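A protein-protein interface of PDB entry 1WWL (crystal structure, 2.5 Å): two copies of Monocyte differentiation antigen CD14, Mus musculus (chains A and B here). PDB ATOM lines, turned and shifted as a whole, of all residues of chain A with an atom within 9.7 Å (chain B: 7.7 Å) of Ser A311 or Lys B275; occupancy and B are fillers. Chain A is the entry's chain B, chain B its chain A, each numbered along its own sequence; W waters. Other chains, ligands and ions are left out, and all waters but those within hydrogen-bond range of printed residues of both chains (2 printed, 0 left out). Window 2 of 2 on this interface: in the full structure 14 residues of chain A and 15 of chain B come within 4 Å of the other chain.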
ATOM      1  N   ARG A 288       0.484  -5.167  13.650  1.00  0.00           N
ATOM      2  CA  ARG A 288      -0.050  -4.071  12.869  1.00  0.00           C
ATOM      3  C   ARG A 288      -1.529  -4.287  12.648  1.00  0.00           C
ATOM      4  O   ARG A 288      -1.953  -5.388  12.297  1.00  0.00           O
ATOM      5  CB  ARG A 288       0.672  -3.969  11.522  1.00  0.00           C
ATOM      6  CG  ARG A 288       1.853  -2.998  11.509  1.00  0.00           C
ATOM      7  CD  ARG A 288       1.387  -1.524  11.435  1.00  0.00           C
ATOM      8  NE  ARG A 288       0.633  -1.092  12.620  1.00  0.00           N
ATOM      9  CZ  ARG A 288      -0.150  -0.014  12.666  1.00  0.00           C
ATOM     10  NH1 ARG A 288      -0.291   0.759  11.596  1.00  0.00           N
ATOM     11  NH2 ARG A 288      -0.810   0.278  13.777  1.00  0.00           N
ATOM     12  N   ASN A 289      -2.306  -3.232  12.870  1.00  0.00           N
ATOM     13  CA  ASN A 289      -3.749  -3.277  12.670  1.00  0.00           C
ATOM     14  C   ASN A 289      -4.000  -3.626  11.209  1.00  0.00           C
ATOM     15  O   ASN A 289      -3.448  -2.989  10.319  1.00  0.00           O
ATOM     16  CB  ASN A 289      -4.363  -1.907  12.988  1.00  0.00           C
ATOM     17  CG  ASN A 289      -5.868  -1.869  12.776  1.00  0.00           C
ATOM     18  OD1 ASN A 289      -6.631  -2.514  13.499  1.00  0.00           O
ATOM     19  ND2 ASN A 289      -6.303  -1.109  11.779  1.00  0.00           N
ATOM     20  N   GLY A 305      -6.563  -8.521  22.253  1.00  0.00           N
ATOM     21  CA  GLY A 305      -5.414  -9.290  22.685  1.00  0.00           C
ATOM     22  C   GLY A 305      -4.188  -9.238  21.803  1.00  0.00           C
ATOM     23  O   GLY A 305      -3.093  -9.541  22.255  1.00  0.00           O
ATOM     24  N   ASN A 306      -4.343  -8.869  20.543  1.00  0.00           N
ATOM     25  CA  ASN A 306      -3.176  -8.822  19.686  1.00  0.00           C
ATOM     26  C   ASN A 306      -2.248  -7.728  20.187  1.00  0.00           C
ATOM     27  O   ASN A 306      -2.651  -6.887  20.975  1.00  0.00           O
ATOM     28  CB  ASN A 306      -3.589  -8.615  18.229  1.00  0.00           C
ATOM     29  CG  ASN A 306      -4.239  -9.858  17.633  1.00  0.00           C
ATOM     30  OD1 ASN A 306      -5.453  -9.919  17.420  1.00  0.00           O
ATOM     31  ND2 ASN A 306      -3.426 -10.861  17.372  1.00  0.00           N
ATOM     32  N   PRO A 307      -0.972  -7.761  19.781  1.00  0.00           N
ATOM     33  CA  PRO A 307      -0.019  -6.739  20.229  1.00  0.00           C
ATOM     34  C   PRO A 307      -0.262  -5.335  19.683  1.00  0.00           C
ATOM     35  O   PRO A 307       0.001  -4.347  20.370  1.00  0.00           O
ATOM     36  CB  PRO A 307       1.326  -7.295  19.767  1.00  0.00           C
ATOM     37  CG  PRO A 307       1.113  -8.770  19.817  1.00  0.00           C
ATOM     38  CD  PRO A 307      -0.263  -8.922  19.213  1.00  0.00           C
ATOM     39  N   PHE A 308      -0.766  -5.232  18.459  1.00  0.00           N
ATOM     40  CA  PHE A 308      -0.971  -3.918  17.883  1.00  0.00           C
ATOM     41  C   PHE A 308      -1.918  -3.079  18.711  1.00  0.00           C
ATOM     42  O   PHE A 308      -1.856  -1.855  18.667  1.00  0.00           O
ATOM     43  CB  PHE A 308      -1.441  -4.033  16.436  1.00  0.00           C
ATOM     44  CG  PHE A 308      -2.920  -4.149  16.272  1.00  0.00           C
ATOM     45  CD1 PHE A 308      -3.732  -3.014  16.322  1.00  0.00           C
ATOM     46  CD2 PHE A 308      -3.500  -5.388  16.012  1.00  0.00           C
ATOM     47  CE1 PHE A 308      -5.101  -3.115  16.110  1.00  0.00           C
ATOM     48  CE2 PHE A 308      -4.869  -5.511  15.797  1.00  0.00           C
ATOM     49  CZ  PHE A 308      -5.676  -4.377  15.845  1.00  0.00           C
ATOM     50  N   LEU A 309      -2.782  -3.736  19.479  1.00  0.00           N
ATOM     51  CA  LEU A 309      -3.724  -3.023  20.329  1.00  0.00           C
ATOM     52  C   LEU A 309      -3.162  -2.719  21.711  1.00  0.00           C
ATOM     53  O   LEU A 309      -3.518  -1.708  22.320  1.00  0.00           O
ATOM     54  CB  LEU A 309      -5.033  -3.802  20.477  1.00  0.00           C
ATOM     55  CG  LEU A 309      -6.011  -3.719  19.309  1.00  0.00           C
ATOM     56  CD1 LEU A 309      -7.148  -4.664  19.563  1.00  0.00           C
ATOM     57  CD2 LEU A 309      -6.531  -2.314  19.135  1.00  0.00           C
ATOM     58  N   ASP A 310      -2.288  -3.578  22.219  1.00  0.00           N
ATOM     59  CA  ASP A 310      -1.742  -3.310  23.533  1.00  0.00           C
ATOM     60  C   ASP A 310      -0.990  -1.989  23.455  1.00  0.00           C
ATOM     61  O   ASP A 310      -0.253  -1.722  22.504  1.00  0.00           O
ATOM     62  CB  ASP A 310      -0.820  -4.453  24.011  1.00  0.00           C
ATOM     63  CG  ASP A 310       0.523  -4.485  23.292  1.00  0.00           C
ATOM     64  OD1 ASP A 310       1.291  -3.506  23.392  1.00  0.00           O
ATOM     65  OD2 ASP A 310       0.821  -5.503  22.632  1.00  0.00           O
ATOM     66  N   SER A 311      -1.225  -1.137  24.437  1.00  0.00           N
ATOM     67  CA  SER A 311      -0.560   0.151  24.500  1.00  0.00           C
ATOM     68  C   SER A 311      -0.085   0.204  25.945  1.00  0.00           C
ATOM     69  O   SER A 311      -0.470   1.091  26.709  1.00  0.00           O
ATOM     70  CB  SER A 311      -1.560   1.274  24.203  1.00  0.00           C
ATOM     71  OG  SER A 311      -0.909   2.519  24.015  1.00  0.00           O
ATOM     72  N   GLU A 312       0.739  -0.780  26.308  1.00  0.00           N
ATOM     73  CA  GLU A 312       1.278  -0.919  27.663  1.00  0.00           C
ATOM     74  C   GLU A 312       2.560  -0.117  27.911  1.00  0.00           C
ATOM     75  O   GLU A 312       2.548   0.758  28.814  1.00  0.00           O
ATOM     76  CB  GLU A 312       1.525  -2.405  27.967  1.00  0.00           C
ATOM     77  OXT GLU A 312       3.564  -0.381  27.205  1.00  0.00           O
ATOM     78  N   PRO B 252     -12.843  11.767  26.027  1.00  0.00           N
ATOM     79  CA  PRO B 252     -12.244  11.556  27.337  1.00  0.00           C
ATOM     80  C   PRO B 252     -11.120  10.526  27.116  1.00  0.00           C
ATOM     81  O   PRO B 252     -11.263   9.581  26.324  1.00  0.00           O
ATOM     82  CB  PRO B 252     -13.403  10.993  28.141  1.00  0.00           C
ATOM     83  CG  PRO B 252     -14.594  11.704  27.555  1.00  0.00           C
ATOM     84  CD  PRO B 252     -14.312  11.661  26.067  1.00  0.00           C
ATOM     85  N   SER B 253      -9.999  10.723  27.796  1.00  0.00           N
ATOM     86  CA  SER B 253      -8.853   9.836  27.644  1.00  0.00           C
ATOM     87  C   SER B 253      -9.117   8.403  28.063  1.00  0.00           C
ATOM     88  O   SER B 253      -8.398   7.516  27.652  1.00  0.00           O
ATOM     89  CB  SER B 253      -7.647  10.381  28.416  1.00  0.00           C
ATOM     90  OG  SER B 253      -7.939  10.493  29.799  1.00  0.00           O
ATOM     91  N   GLN B 254     -10.148   8.158  28.861  1.00  0.00           N
ATOM     92  CA  GLN B 254     -10.439   6.793  29.302  1.00  0.00           C
ATOM     93  C   GLN B 254     -11.515   6.067  28.502  1.00  0.00           C
ATOM     94  O   GLN B 254     -11.939   4.967  28.862  1.00  0.00           O
ATOM     95  CB  GLN B 254     -10.846   6.803  30.767  1.00  0.00           C
ATOM     96  CG  GLN B 254      -9.684   7.036  31.732  1.00  0.00           C
ATOM     97  CD  GLN B 254     -10.081   6.735  33.175  1.00  0.00           C
ATOM     98  OE1 GLN B 254     -10.813   7.506  33.811  1.00  0.00           O
ATOM     99  NE2 GLN B 254      -9.615   5.588  33.693  1.00  0.00           N
ATOM    100  N   LEU B 255     -11.953   6.673  27.411  1.00  0.00           N
ATOM    101  CA  LEU B 255     -13.013   6.088  26.614  1.00  0.00           C
ATOM    102  C   LEU B 255     -12.527   4.867  25.845  1.00  0.00           C
ATOM    103  O   LEU B 255     -11.625   4.958  25.019  1.00  0.00           O
ATOM    104  CB  LEU B 255     -13.583   7.146  25.646  1.00  0.00           C
ATOM    105  CG  LEU B 255     -14.653   6.618  24.700  1.00  0.00           C
ATOM    106  CD1 LEU B 255     -15.898   6.280  25.460  1.00  0.00           C
ATOM    107  CD2 LEU B 255     -14.949   7.625  23.652  1.00  0.00           C
ATOM    108  N   ASN B 256     -13.143   3.723  26.105  1.00  0.00           N
ATOM    109  CA  ASN B 256     -12.735   2.523  25.412  1.00  0.00           C
ATOM    110  C   ASN B 256     -13.883   1.742  24.771  1.00  0.00           C
ATOM    111  O   ASN B 256     -13.638   0.745  24.085  1.00  0.00           O
ATOM    112  CB  ASN B 256     -11.949   1.614  26.359  1.00  0.00           C
ATOM    113  CG  ASN B 256     -12.746   1.199  27.545  1.00  0.00           C
ATOM    114  OD1 ASN B 256     -12.297   1.329  28.683  1.00  0.00           O
ATOM    115  ND2 ASN B 256     -13.940   0.687  27.305  1.00  0.00           N
ATOM    116  N   SER B 257     -15.121   2.190  24.985  1.00  0.00           N
ATOM    117  CA  SER B 257     -16.295   1.521  24.426  1.00  0.00           C
ATOM    118  C   SER B 257     -17.383   2.509  23.915  1.00  0.00           C
ATOM    119  O   SER B 257     -17.998   3.251  24.698  1.00  0.00           O
ATOM    120  CB  SER B 257     -16.885   0.578  25.470  1.00  0.00           C
ATOM    121  OG  SER B 257     -18.031  -0.025  24.910  1.00  0.00           O
ATOM    122  N   LEU B 272     -14.206  10.159  15.399  1.00  0.00           N
ATOM    123  CA  LEU B 272     -14.354   9.038  16.328  1.00  0.00           C
ATOM    124  C   LEU B 272     -13.043   8.957  17.109  1.00  0.00           C
ATOM    125  O   LEU B 272     -12.052   9.542  16.700  1.00  0.00           O
ATOM    126  CB  LEU B 272     -14.615   7.724  15.592  1.00  0.00           C
ATOM    127  CG  LEU B 272     -16.005   7.644  14.944  1.00  0.00           C
ATOM    128  CD1 LEU B 272     -16.268   6.234  14.495  1.00  0.00           C
ATOM    129  CD2 LEU B 272     -17.098   8.032  15.935  1.00  0.00           C
ATOM    130  N   PRO B 273     -13.029   8.275  18.258  1.00  0.00           N
ATOM    131  CA  PRO B 273     -11.770   8.193  18.998  1.00  0.00           C
ATOM    132  C   PRO B 273     -10.790   7.400  18.121  1.00  0.00           C
ATOM    133  O   PRO B 273     -11.221   6.667  17.210  1.00  0.00           O
ATOM    134  CB  PRO B 273     -12.159   7.440  20.271  1.00  0.00           C
ATOM    135  CG  PRO B 273     -13.588   7.781  20.439  1.00  0.00           C
ATOM    136  CD  PRO B 273     -14.120   7.655  19.025  1.00  0.00           C
ATOM    137  N   ALA B 274      -9.492   7.536  18.392  1.00  0.00           N
ATOM    138  CA  ALA B 274      -8.480   6.854  17.594  1.00  0.00           C
ATOM    139  C   ALA B 274      -8.343   5.366  17.898  1.00  0.00           C
ATOM    140  O   ALA B 274      -8.117   4.561  16.994  1.00  0.00           O
ATOM    141  CB  ALA B 274      -7.130   7.541  17.778  1.00  0.00           C
ATOM    142  N   LYS B 275      -8.469   4.998  19.167  1.00  0.00           N
ATOM    143  CA  LYS B 275      -8.339   3.594  19.571  1.00  0.00           C
ATOM    144  C   LYS B 275      -9.494   3.252  20.497  1.00  0.00           C
ATOM    145  O   LYS B 275      -9.843   4.049  21.373  1.00  0.00           O
ATOM    146  CB  LYS B 275      -6.985   3.361  20.282  1.00  0.00           C
ATOM    147  CG  LYS B 275      -6.914   2.065  21.134  1.00  0.00           C
ATOM    148  CD  LYS B 275      -5.547   1.340  21.040  1.00  0.00           C
ATOM    149  CE  LYS B 275      -4.865   1.118  22.411  1.00  0.00           C
ATOM    150  NZ  LYS B 275      -4.177   2.343  22.960  1.00  0.00           N
ATOM    151  N   LEU B 276     -10.097   2.087  20.292  1.00  0.00           N
ATOM    152  CA  LEU B 276     -11.221   1.658  21.108  1.00  0.00           C
ATOM    153  C   LEU B 276     -11.153   0.141  21.376  1.00  0.00           C
ATOM    154  O   LEU B 276     -10.622  -0.615  20.572  1.00  0.00           O
ATOM    155  CB  LEU B 276     -12.516   2.010  20.359  1.00  0.00           C
ATOM    156  CG  LEU B 276     -13.609   3.029  20.783  1.00  0.00           C
ATOM    157  CD1 LEU B 276     -13.098   4.146  21.677  1.00  0.00           C
ATOM    158  CD2 LEU B 276     -14.237   3.601  19.506  1.00  0.00           C
ATOM    159  N   SER B 277     -11.676  -0.311  22.509  1.00  0.00           N
ATOM    160  CA  SER B 277     -11.699  -1.736  22.793  1.00  0.00           C
ATOM    161  C   SER B 277     -12.892  -2.279  22.030  1.00  0.00           C
ATOM    162  O   SER B 277     -12.786  -3.316  21.381  1.00  0.00           O
ATOM    163  CB  SER B 277     -11.884  -1.990  24.270  1.00  0.00           C
ATOM    164  OG  SER B 277     -10.948  -1.227  24.979  1.00  0.00           O
ATOM    165  N   VAL B 278     -14.033  -1.588  22.129  1.00  0.00           N
ATOM    166  CA  VAL B 278     -15.224  -1.988  21.378  1.00  0.00           C
ATOM    167  C   VAL B 278     -15.950  -0.823  20.688  1.00  0.00           C
ATOM    168  O   VAL B 278     -16.084   0.282  21.236  1.00  0.00           O
ATOM    169  CB  VAL B 278     -16.244  -2.834  22.257  1.00  0.00           C
ATOM    170  CG1 VAL B 278     -15.718  -3.048  23.654  1.00  0.00           C
ATOM    171  CG2 VAL B 278     -17.626  -2.210  22.254  1.00  0.00           C
ATOM    172  N   LEU B 295     -11.910   3.994   9.982  1.00  0.00           N
ATOM    173  CA  LEU B 295     -12.221   3.383  11.270  1.00  0.00           C
ATOM    174  C   LEU B 295     -11.090   3.471  12.276  1.00  0.00           C
ATOM    175  O   LEU B 295      -9.928   3.610  11.897  1.00  0.00           O
ATOM    176  CB  LEU B 295     -12.552   1.909  11.022  1.00  0.00           C
ATOM    177  CG  LEU B 295     -13.846   1.183  11.407  1.00  0.00           C
ATOM    178  CD1 LEU B 295     -15.038   2.114  11.568  1.00  0.00           C
ATOM    179  CD2 LEU B 295     -14.094   0.139  10.335  1.00  0.00           C
ATOM    180  N   PRO B 296     -11.417   3.417  13.581  1.00  0.00           N
ATOM    181  CA  PRO B 296     -10.399   3.475  14.647  1.00  0.00           C
ATOM    182  C   PRO B 296      -9.840   2.064  14.797  1.00  0.00           C
ATOM    183  O   PRO B 296     -10.322   1.124  14.148  1.00  0.00           O
ATOM    184  CB  PRO B 296     -11.198   3.855  15.897  1.00  0.00           C
ATOM    185  CG  PRO B 296     -12.498   4.390  15.372  1.00  0.00           C
ATOM    186  CD  PRO B 296     -12.772   3.615  14.127  1.00  0.00           C
ATOM    187  N   GLN B 297      -8.826   1.911  15.646  1.00  0.00           N
ATOM    188  CA  GLN B 297      -8.273   0.594  15.906  1.00  0.00           C
ATOM    189  C   GLN B 297      -9.255   0.021  16.904  1.00  0.00           C
ATOM    190  O   GLN B 297      -9.439   0.576  17.991  1.00  0.00           O
ATOM    191  CB  GLN B 297      -6.900   0.692  16.542  1.00  0.00           C
ATOM    192  CG  GLN B 297      -5.842   1.137  15.618  1.00  0.00           C
ATOM    193  CD  GLN B 297      -4.456   1.045  16.249  1.00  0.00           C
ATOM    194  OE1 GLN B 297      -3.450   1.366  15.606  1.00  0.00           O
ATOM    195  NE2 GLN B 297      -4.397   0.603  17.512  1.00  0.00           N
ATOM    196  N   VAL B 298      -9.872  -1.095  16.554  1.00  0.00           N
ATOM    197  CA  VAL B 298     -10.891  -1.677  17.419  1.00  0.00           C
ATOM    198  C   VAL B 298     -10.595  -3.123  17.788  1.00  0.00           C
ATOM    199  O   VAL B 298     -10.257  -3.913  16.916  1.00  0.00           O
ATOM    200  CB  VAL B 298     -12.291  -1.625  16.697  1.00  0.00           C
ATOM    201  CG1 VAL B 298     -13.331  -2.306  17.519  1.00  0.00           C
ATOM    202  CG2 VAL B 298     -12.708  -0.187  16.435  1.00  0.00           C
ATOM    203  N   GLY B 299     -10.725  -3.465  19.069  1.00  0.00           N
ATOM    204  CA  GLY B 299     -10.525  -4.842  19.479  1.00  0.00           C
ATOM    205  C   GLY B 299     -11.788  -5.652  19.162  1.00  0.00           C
ATOM    206  O   GLY B 299     -11.744  -6.825  18.784  1.00  0.00           O
HETATM  207  O   HOH W   1      -2.771   0.586  20.471  1.00  0.00           O
HETATM  208  O   HOH W   2      -9.277  -2.637  14.333  1.00  0.00           O
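No position is printed for both chains.
Of the 6 pairs that touch across the chains among the printed residues, none has its exchanged pair printed and touching as well.
Printed residues of chain B that touch a printed residue of chain A: Lys B275, Gln B297 and Gly B299.
Hydrophobic or aromatic side chains of chain A that line the printed part of chain B: Phe A308 and Leu A309.
Among the printed residues, 6 pairs touch across the chains.
Among the printed residues, no Asp or Glu carboxylate lies within 4 Å of a Lys or Arg side-chain nitrogen of the other chain.
Of the printed residues of chain A, Lys B275 touches Leu A309 (3.1 Å) and Ser A311 (3.1 Å).
No residue of chain A comes within 4 Å of Leu B276.
Of the printed residues of chain A, Gly B299 touches Leu A309 (3.4 Å).
Printed residues of chain B within 4 Å of Arg A288: Gln B297 (3.4 Å).
Of the printed residues of chain B, Phe A308 touches Gln B297 (3.7 Å).
Printed residues of chain A within 4 Å of Gln B297: Arg A288, Phe A308 and Leu A309.
Gln B254 touches none of the printed residues of chain A.
The nearest residue of chain A that does not touch Lys B275 is Asp A310 (5.1 Å).
O of Ala B274 lies within hydrogen-bond range of N of Gln B297, 3.1 Å away.
The backbone NH (N) of Leu B276 lies within hydrogen-bond range of the backbone carbonyl oxygen (O) of Gln B297 (2.8 Å).
The backbone NH (N) of Gly B299 lies within hydrogen-bond range of the backbone carbonyl oxygen (O) of Leu B276, 3.2 Å away.
O of Ser B277 sits at hydrogen-bond distance from N of Gly B299 (3.1 Å).
Water W2 lies within hydrogen-bond range of N of Val B298 and OD1 of Asn A289.
Water W1 lies within hydrogen-bond range of the backbone carbonyl oxygen (O) of Leu A309 (3.0 Å), the backbone carbonyl oxygen (O) of Phe A308 (3.2 Å), the side-chain amino group (NZ) of Lys B275 (3.4 Å) and the side-chain amide nitrogen (NE2) of Gln B297 (3.4 Å).
Phe A308 touches Gln B297.
CE of Lys B275 touches O of Leu A309 (3.1 Å).
Leu A309 touches Gln B297 (CD2 to NE2, 3.96 Å).
Gly B299 touches Leu A309.
The side-chain amino group (NZ) of Lys B275 lies close to the side-chain hydroxyl (OG) of Ser A311, at 3.4 Å.
OE1 of Gln B297 lies within hydrogen-bond range of NH2 of Arg A288 (3.4 Å).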
